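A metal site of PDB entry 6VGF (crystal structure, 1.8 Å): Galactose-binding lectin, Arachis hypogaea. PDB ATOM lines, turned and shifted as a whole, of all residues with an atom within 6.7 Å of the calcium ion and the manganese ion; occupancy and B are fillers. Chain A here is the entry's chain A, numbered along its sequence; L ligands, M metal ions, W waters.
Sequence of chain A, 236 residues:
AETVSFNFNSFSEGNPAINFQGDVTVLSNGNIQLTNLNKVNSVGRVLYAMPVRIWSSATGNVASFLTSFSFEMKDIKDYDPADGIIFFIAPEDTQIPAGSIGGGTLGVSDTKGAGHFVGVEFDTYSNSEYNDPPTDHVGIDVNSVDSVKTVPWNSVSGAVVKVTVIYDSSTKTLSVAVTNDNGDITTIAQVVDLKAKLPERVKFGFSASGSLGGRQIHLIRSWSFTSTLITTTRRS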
ATOM      1  N   ASP A  83      -3.771 -33.553  26.708  1.00  0.00           N
ATOM      2  CA  ASP A  83      -4.018 -32.293  25.992  1.00  0.00           C
ATOM      3  C   ASP A  83      -3.259 -31.065  26.471  1.00  0.00           C
ATOM      4  O   ASP A  83      -3.247 -30.047  25.772  1.00  0.00           O
ATOM      5  CB  ASP A  83      -5.500 -31.975  25.997  1.00  0.00           C
ATOM      6  CG  ASP A  83      -6.211 -32.718  24.895  1.00  0.00           C
ATOM      7  OD1 ASP A  83      -6.250 -32.189  23.756  1.00  0.00           O
ATOM      8  OD2 ASP A  83      -6.683 -33.872  25.153  1.00  0.00           O
ATOM      9  N   GLY A 103     -10.362 -33.546  27.073  1.00  0.00           N
ATOM     10  CA  GLY A 103      -9.728 -33.162  25.814  1.00  0.00           C
ATOM     11  C   GLY A 103      -9.241 -31.715  25.747  1.00  0.00           C
ATOM     12  O   GLY A 103      -8.518 -31.258  26.642  1.00  0.00           O
ATOM     13  N   GLY A 104      -9.663 -31.003  24.695  1.00  0.00           N
ATOM     14  CA  GLY A 104      -9.303 -29.617  24.417  1.00  0.00           C
ATOM     15  C   GLY A 104      -9.881 -28.587  25.378  1.00  0.00           C
ATOM     16  O   GLY A 104      -9.468 -27.427  25.338  1.00  0.00           O
ATOM     17  N   THR A 105     -10.863 -29.003  26.218  1.00  0.00           N
ATOM     18  CA  THR A 105     -11.501 -28.124  27.203  1.00  0.00           C
ATOM     19  C   THR A 105     -10.547 -27.836  28.367  1.00  0.00           C
ATOM     20  O   THR A 105     -10.847 -26.972  29.190  1.00  0.00           O
ATOM     21  CB  THR A 105     -12.846 -28.726  27.719  1.00  0.00           C
ATOM     22  OG1 THR A 105     -12.613 -29.788  28.658  1.00  0.00           O
ATOM     23  CG2 THR A 105     -13.770 -29.161  26.597  1.00  0.00           C
ATOM     24  N   LEU A 106      -9.478 -28.659  28.496  1.00  0.00           N
ATOM     25  CA  LEU A 106      -8.425 -28.606  29.520  1.00  0.00           C
ATOM     26  C   LEU A 106      -9.022 -28.703  30.950  1.00  0.00           C
ATOM     27  O   LEU A 106      -8.362 -28.344  31.930  1.00  0.00           O
ATOM     28  CB  LEU A 106      -7.556 -27.317  29.362  1.00  0.00           C
ATOM     29  CG  LEU A 106      -6.793 -27.183  28.047  1.00  0.00           C
ATOM     30  CD1 LEU A 106      -6.059 -25.831  27.995  1.00  0.00           C
ATOM     31  CD2 LEU A 106      -5.824 -28.343  27.801  1.00  0.00           C
ATOM     32  N   GLU A 121      -2.495 -21.414  29.667  1.00  0.00           N
ATOM     33  CA  GLU A 121      -2.470 -22.802  29.172  1.00  0.00           C
ATOM     34  C   GLU A 121      -1.149 -23.156  28.503  1.00  0.00           C
ATOM     35  O   GLU A 121      -0.513 -22.314  27.864  1.00  0.00           O
ATOM     36  CB  GLU A 121      -3.628 -23.069  28.197  1.00  0.00           C
ATOM     37  CG  GLU A 121      -3.619 -22.128  27.014  1.00  0.00           C
ATOM     38  CD  GLU A 121      -4.509 -22.611  25.899  1.00  0.00           C
ATOM     39  OE1 GLU A 121      -5.732 -22.703  26.140  1.00  0.00           O
ATOM     40  OE2 GLU A 121      -3.989 -22.908  24.812  1.00  0.00           O
ATOM     41  N   ASP A 123      -0.624 -25.825  26.056  1.00  0.00           N
ATOM     42  CA  ASP A 123      -1.428 -26.638  25.157  1.00  0.00           C
ATOM     43  C   ASP A 123      -0.593 -27.438  24.171  1.00  0.00           C
ATOM     44  O   ASP A 123       0.168 -26.860  23.397  1.00  0.00           O
ATOM     45  CB  ASP A 123      -2.381 -25.685  24.422  1.00  0.00           C
ATOM     46  CG  ASP A 123      -3.550 -26.377  23.760  1.00  0.00           C
ATOM     47  OD1 ASP A 123      -3.536 -27.631  23.684  1.00  0.00           O
ATOM     48  OD2 ASP A 123      -4.507 -25.682  23.391  1.00  0.00           O
ATOM     49  N   THR A 124      -0.764 -28.788  24.196  1.00  0.00           N
ATOM     50  CA  THR A 124       0.050 -29.700  23.388  1.00  0.00           C
ATOM     51  C   THR A 124      -0.724 -30.392  22.245  1.00  0.00           C
ATOM     52  O   THR A 124      -0.177 -31.318  21.623  1.00  0.00           O
ATOM     53  CB  THR A 124       0.716 -30.748  24.288  1.00  0.00           C
ATOM     54  OG1 THR A 124      -0.247 -31.682  24.766  1.00  0.00           O
ATOM     55  CG2 THR A 124       1.446 -30.119  25.456  1.00  0.00           C
ATOM     56  N   TYR A 125      -1.936 -29.924  21.922  1.00  0.00           N
ATOM     57  CA  TYR A 125      -2.758 -30.472  20.831  1.00  0.00           C
ATOM     58  C   TYR A 125      -3.602 -29.366  20.190  1.00  0.00           C
ATOM     59  O   TYR A 125      -4.286 -28.623  20.892  1.00  0.00           O
ATOM     60  CB  TYR A 125      -3.661 -31.630  21.316  1.00  0.00           C
ATOM     61  CG  TYR A 125      -4.434 -32.234  20.158  1.00  0.00           C
ATOM     62  CD1 TYR A 125      -5.678 -31.735  19.789  1.00  0.00           C
ATOM     63  CD2 TYR A 125      -3.875 -33.235  19.376  1.00  0.00           C
ATOM     64  CE1 TYR A 125      -6.350 -32.209  18.666  1.00  0.00           C
ATOM     65  CE2 TYR A 125      -4.556 -33.756  18.272  1.00  0.00           C
ATOM     66  CZ  TYR A 125      -5.780 -33.228  17.907  1.00  0.00           C
ATOM     67  OH  TYR A 125      -6.447 -33.745  16.833  1.00  0.00           O
ATOM     68  N   SER A 126      -3.593 -29.294  18.842  1.00  0.00           N
ATOM     69  CA  SER A 126      -4.315 -28.273  18.081  1.00  0.00           C
ATOM     70  C   SER A 126      -5.777 -28.652  17.841  1.00  0.00           C
ATOM     71  O   SER A 126      -6.069 -29.496  16.995  1.00  0.00           O
ATOM     72  CB  SER A 126      -3.606 -28.002  16.751  1.00  0.00           C
ATOM     73  OG  SER A 126      -4.182 -26.872  16.113  1.00  0.00           O
ATOM     74  N   ASN A 127      -6.699 -28.022  18.611  1.00  0.00           N
ATOM     75  CA  ASN A 127      -8.146 -28.176  18.505  1.00  0.00           C
ATOM     76  C   ASN A 127      -8.719 -27.090  17.601  1.00  0.00           C
ATOM     77  O   ASN A 127      -8.876 -25.943  18.024  1.00  0.00           O
ATOM     78  CB  ASN A 127      -8.811 -28.116  19.888  1.00  0.00           C
ATOM     79  CG  ASN A 127      -8.374 -29.216  20.807  1.00  0.00           C
ATOM     80  OD1 ASN A 127      -7.269 -29.188  21.358  1.00  0.00           O
ATOM     81  ND2 ASN A 127      -9.209 -30.216  20.973  1.00  0.00           N
ATOM     82  N   TYR A 130     -11.544 -24.871  18.756  1.00  0.00           N
ATOM     83  CA  TYR A 130     -11.230 -23.781  19.697  1.00  0.00           C
ATOM     84  C   TYR A 130     -10.230 -22.780  19.077  1.00  0.00           C
ATOM     85  O   TYR A 130      -9.649 -21.957  19.784  1.00  0.00           O
ATOM     86  CB  TYR A 130     -10.702 -24.343  21.029  1.00  0.00           C
ATOM     87  CG  TYR A 130     -11.628 -25.383  21.647  1.00  0.00           C
ATOM     88  CD1 TYR A 130     -12.992 -25.139  21.767  1.00  0.00           C
ATOM     89  CD2 TYR A 130     -11.125 -26.566  22.158  1.00  0.00           C
ATOM     90  CE1 TYR A 130     -13.848 -26.092  22.305  1.00  0.00           C
ATOM     91  CE2 TYR A 130     -11.974 -27.537  22.688  1.00  0.00           C
ATOM     92  CZ  TYR A 130     -13.337 -27.285  22.767  1.00  0.00           C
ATOM     93  OH  TYR A 130     -14.167 -28.215  23.326  1.00  0.00           O
ATOM     94  N   ASN A 131     -10.060 -22.860  17.740  1.00  0.00           N
ATOM     95  CA  ASN A 131      -9.181 -22.025  16.916  1.00  0.00           C
ATOM     96  C   ASN A 131      -7.736 -22.021  17.432  1.00  0.00           C
ATOM     97  O   ASN A 131      -7.081 -20.985  17.442  1.00  0.00           O
ATOM     98  CB  ASN A 131      -9.745 -20.585  16.792  1.00  0.00           C
ATOM     99  CG  ASN A 131     -11.022 -20.514  15.997  1.00  0.00           C
ATOM    100  OD1 ASN A 131     -11.091 -20.932  14.841  1.00  0.00           O
ATOM    101  ND2 ASN A 131     -12.068 -19.974  16.622  1.00  0.00           N
ATOM    102  N   ASP A 132      -7.257 -23.201  17.864  1.00  0.00           N
ATOM    103  CA  ASP A 132      -5.885 -23.364  18.348  1.00  0.00           C
ATOM    104  C   ASP A 132      -4.877 -23.088  17.247  1.00  0.00           C
ATOM    105  O   ASP A 132      -5.137 -23.496  16.107  1.00  0.00           O
ATOM    106  CB  ASP A 132      -5.642 -24.805  18.842  1.00  0.00           C
ATOM    107  CG  ASP A 132      -5.902 -25.042  20.311  1.00  0.00           C
ATOM    108  OD1 ASP A 132      -5.907 -24.061  21.083  1.00  0.00           O
ATOM    109  OD2 ASP A 132      -6.043 -26.217  20.702  1.00  0.00           O
ATOM    110  N   PRO A 133      -3.700 -22.508  17.541  1.00  0.00           N
ATOM    111  CA  PRO A 133      -2.684 -22.360  16.471  1.00  0.00           C
ATOM    112  C   PRO A 133      -2.172 -23.751  16.024  1.00  0.00           C
ATOM    113  O   PRO A 133      -2.457 -24.735  16.719  1.00  0.00           O
ATOM    114  CB  PRO A 133      -1.600 -21.486  17.120  1.00  0.00           C
ATOM    115  CG  PRO A 133      -1.770 -21.675  18.587  1.00  0.00           C
ATOM    116  CD  PRO A 133      -3.217 -21.977  18.839  1.00  0.00           C
ATOM    117  N   HIS A 137       1.612 -24.459  22.126  1.00  0.00           N
ATOM    118  CA  HIS A 137       1.572 -23.046  22.448  1.00  0.00           C
ATOM    119  C   HIS A 137       1.238 -22.763  23.913  1.00  0.00           C
ATOM    120  O   HIS A 137       0.583 -23.556  24.584  1.00  0.00           O
ATOM    121  CB  HIS A 137       0.528 -22.330  21.565  1.00  0.00           C
ATOM    122  CG  HIS A 137      -0.836 -22.968  21.626  1.00  0.00           C
ATOM    123  ND1 HIS A 137      -1.120 -24.160  20.938  1.00  0.00           N
ATOM    124  CD2 HIS A 137      -1.946 -22.571  22.278  1.00  0.00           C
ATOM    125  CE1 HIS A 137      -2.390 -24.413  21.184  1.00  0.00           C
ATOM    126  NE2 HIS A 137      -2.921 -23.485  21.999  1.00  0.00           N
ATOM    127  N   VAL A 138       1.629 -21.574  24.337  1.00  0.00           N
ATOM    128  CA  VAL A 138       1.270 -21.008  25.617  1.00  0.00           C
ATOM    129  C   VAL A 138       0.185 -19.999  25.291  1.00  0.00           C
ATOM    130  O   VAL A 138       0.320 -19.240  24.316  1.00  0.00           O
ATOM    131  CB  VAL A 138       2.457 -20.425  26.434  1.00  0.00           C
ATOM    132  CG1 VAL A 138       1.978 -19.848  27.765  1.00  0.00           C
ATOM    133  CG2 VAL A 138       3.528 -21.476  26.686  1.00  0.00           C
ATOM    134  N   GLY A 139      -0.927 -20.059  26.002  1.00  0.00           N
ATOM    135  CA  GLY A 139      -2.022 -19.156  25.721  1.00  0.00           C
ATOM    136  C   GLY A 139      -2.505 -18.414  26.942  1.00  0.00           C
ATOM    137  O   GLY A 139      -2.298 -18.886  28.050  1.00  0.00           O
ATOM    138  N   ASP A 141      -5.945 -17.112  28.508  1.00  0.00           N
ATOM    139  CA  ASP A 141      -7.363 -17.459  28.364  1.00  0.00           C
ATOM    140  C   ASP A 141      -8.265 -16.643  29.255  1.00  0.00           C
ATOM    141  O   ASP A 141      -8.022 -16.541  30.441  1.00  0.00           O
ATOM    142  CB  ASP A 141      -7.574 -18.947  28.663  1.00  0.00           C
ATOM    143  CG  ASP A 141      -6.895 -19.904  27.706  1.00  0.00           C
ATOM    144  OD1 ASP A 141      -6.407 -19.455  26.643  1.00  0.00           O
ATOM    145  OD2 ASP A 141      -6.914 -21.118  27.981  1.00  0.00           O
ATOM    146  N   VAL A 145     -11.268 -21.374  26.127  1.00  0.00           N
ATOM    147  CA  VAL A 145     -10.076 -22.075  25.678  1.00  0.00           C
ATOM    148  C   VAL A 145      -9.769 -21.627  24.221  1.00  0.00           C
ATOM    149  O   VAL A 145      -8.798 -22.092  23.622  1.00  0.00           O
ATOM    150  CB  VAL A 145     -10.077 -23.627  25.838  1.00  0.00           C
ATOM    151  CG1 VAL A 145      -9.961 -24.021  27.316  1.00  0.00           C
ATOM    152  CG2 VAL A 145     -11.309 -24.248  25.197  1.00  0.00           C
ATOM    153  N   ASP A 146     -10.565 -20.691  23.663  1.00  0.00           N
ATOM    154  CA  ASP A 146     -10.234 -19.988  22.414  1.00  0.00           C
ATOM    155  C   ASP A 146      -9.452 -18.770  22.938  1.00  0.00           C
ATOM    156  O   ASP A 146     -10.047 -17.770  23.325  1.00  0.00           O
ATOM    157  CB  ASP A 146     -11.480 -19.662  21.573  1.00  0.00           C
ATOM    158  CG  ASP A 146     -11.205 -19.020  20.200  1.00  0.00           C
ATOM    159  OD1 ASP A 146     -10.113 -18.441  20.004  1.00  0.00           O
ATOM    160  OD2 ASP A 146     -12.092 -19.072  19.323  1.00  0.00           O
ATOM    161  N   SER A 147      -8.136 -18.930  23.056  1.00  0.00           N
ATOM    162  CA  SER A 147      -7.242 -17.964  23.694  1.00  0.00           C
ATOM    163  C   SER A 147      -7.350 -16.535  23.166  1.00  0.00           C
ATOM    164  O   SER A 147      -7.462 -16.304  21.951  1.00  0.00           O
ATOM    165  CB  SER A 147      -5.785 -18.407  23.579  1.00  0.00           C
ATOM    166  OG  SER A 147      -5.527 -19.661  24.163  1.00  0.00           O
ATOM    167  N   THR A 150      -1.879 -16.215  21.988  1.00  0.00           N
ATOM    168  CA  THR A 150      -0.990 -17.377  22.093  1.00  0.00           C
ATOM    169  C   THR A 150       0.400 -17.005  21.608  1.00  0.00           C
ATOM    170  O   THR A 150       0.579 -16.013  20.905  1.00  0.00           O
ATOM    171  CB  THR A 150      -1.484 -18.631  21.306  1.00  0.00           C
ATOM    172  OG1 THR A 150      -1.429 -18.412  19.904  1.00  0.00           O
ATOM    173  CG2 THR A 150      -2.835 -19.127  21.738  1.00  0.00           C
HETATM  174  C1  LIG L   1      -9.472 -35.467  20.184  1.00  0.00           C
HETATM  175  S1  LIG L   1     -10.927 -36.531  20.100  1.00  0.00           S
HETATM  176  C2  LIG L   1      -9.650 -34.380  21.241  1.00  0.00           C
HETATM  177  O1  LIG L   1     -10.733 -33.525  20.896  1.00  0.00           O
HETATM  178  C3  LIG L   1      -8.381 -33.544  21.383  1.00  0.00           C
HETATM  179  O2  LIG L   1      -8.537 -32.606  22.428  1.00  0.00           O
HETATM  180  C4  LIG L   1      -7.169 -34.456  21.604  1.00  0.00           C
HETATM  181  O3  LIG L   1      -7.228 -35.087  22.882  1.00  0.00           O
HETATM  182  C5  LIG L   1      -7.110 -35.476  20.474  1.00  0.00           C
HETATM  183  O4  LIG L   1      -8.319 -36.254  20.464  1.00  0.00           O
HETATM  184  C6  LIG L   1      -5.957 -36.445  20.563  1.00  0.00           C
HETATM  185  O5  LIG L   1      -5.717 -37.063  19.291  1.00  0.00           O
HETATM  186  C7  LIG L   1     -10.791 -37.160  18.397  1.00  0.00           C
HETATM  187  C8  LIG L   1     -11.526 -38.489  18.216  1.00  0.00           C
HETATM  188  O6  LIG L   1     -11.038 -39.450  19.155  1.00  0.00           O
HETATM  189  C9  LIG L   1     -11.320 -38.965  16.782  1.00  0.00           C
HETATM  190  O7  LIG L   1     -12.001 -40.189  16.543  1.00  0.00           O
HETATM  191  C10 LIG L   1     -11.766 -37.899  15.777  1.00  0.00           C
HETATM  192  O8  LIG L   1     -11.376 -38.300  14.466  1.00  0.00           O
HETATM  193  C11 LIG L   1     -11.140 -36.533  16.091  1.00  0.00           C
HETATM  194  O9  LIG L   1     -11.300 -36.192  17.478  1.00  0.00           O
HETATM  195  C12 LIG L   1     -11.853 -35.388  15.401  1.00  0.00           C
HETATM  196  C13 LIG L   1     -29.662 -18.956  13.235  1.00  0.00           C
HETATM  197 CA    CA M   1      -5.577 -27.730  22.386  1.00  0.00          CA
HETATM  198 MN    MN M   2      -4.764 -23.655  22.907  1.00  0.00          MN
HETATM  199  O   HOH W   1      -5.616 -29.406  23.907  1.00  0.00           O
HETATM  200  O   HOH W   2      -6.911 -23.877  24.075  1.00  0.00           O
HETATM  201  O   HOH W   3      -7.413 -26.733  23.685  1.00  0.00           O
HETATM  202  O   HOH W   4      -5.042 -21.649  22.291  1.00  0.00           O
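The calcium ion is bound by O of Tyr 125, water W1, OD2 of Asp 132, OD1 of Asp 123, OD1 of Asn 127, water W3 and OD2 of Asp 123.
The calcium ion has seven donor atoms within binding distance.
The manganese ion is bound by NE2 of His 137, OD2 of Asp 123, water W4, OE2 of Glu 121, OD1 of Asp 132 and water W2.
The manganese ion has six donor atoms within binding distance.
Water W2 lies within hydrogen-bond range of the backbone carbonyl oxygen of Val 145 (2.6 Å) and the side-chain carboxylate of Glu 121 (2.7 Å).
Within 4 Å of the manganese ion: Glu 121, Asp 123, Asp 132 and His 137.
Four residues have an atom within 4 Å of the calcium ion: Asp 123, Tyr 125, Asn 127 and Asp 132.
The nearest printed residue that does not touch the calcium ion is Ser 126 (4.4 Å).
The side-chain carboxylate (OD2) of Asp 141 lies close to the side-chain carboxylate (OE1) of Glu 121.
O of Glu 121 lies within hydrogen-bond range of N of Gly 139, at 3.0 Å.
The side-chain carboxylate (OD2) of Asp 83 lies within hydrogen-bond range of an oxygen (O3) of the ligand (2.6 Å).
The backbone NH of Gly 104 sits at hydrogen-bond distance from an oxygen (O2) of the ligand, at 3.0 Å.
ND2 of Asn 127 is in hydrogen-bond range of O2 of the ligand, 2.9 Å away.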
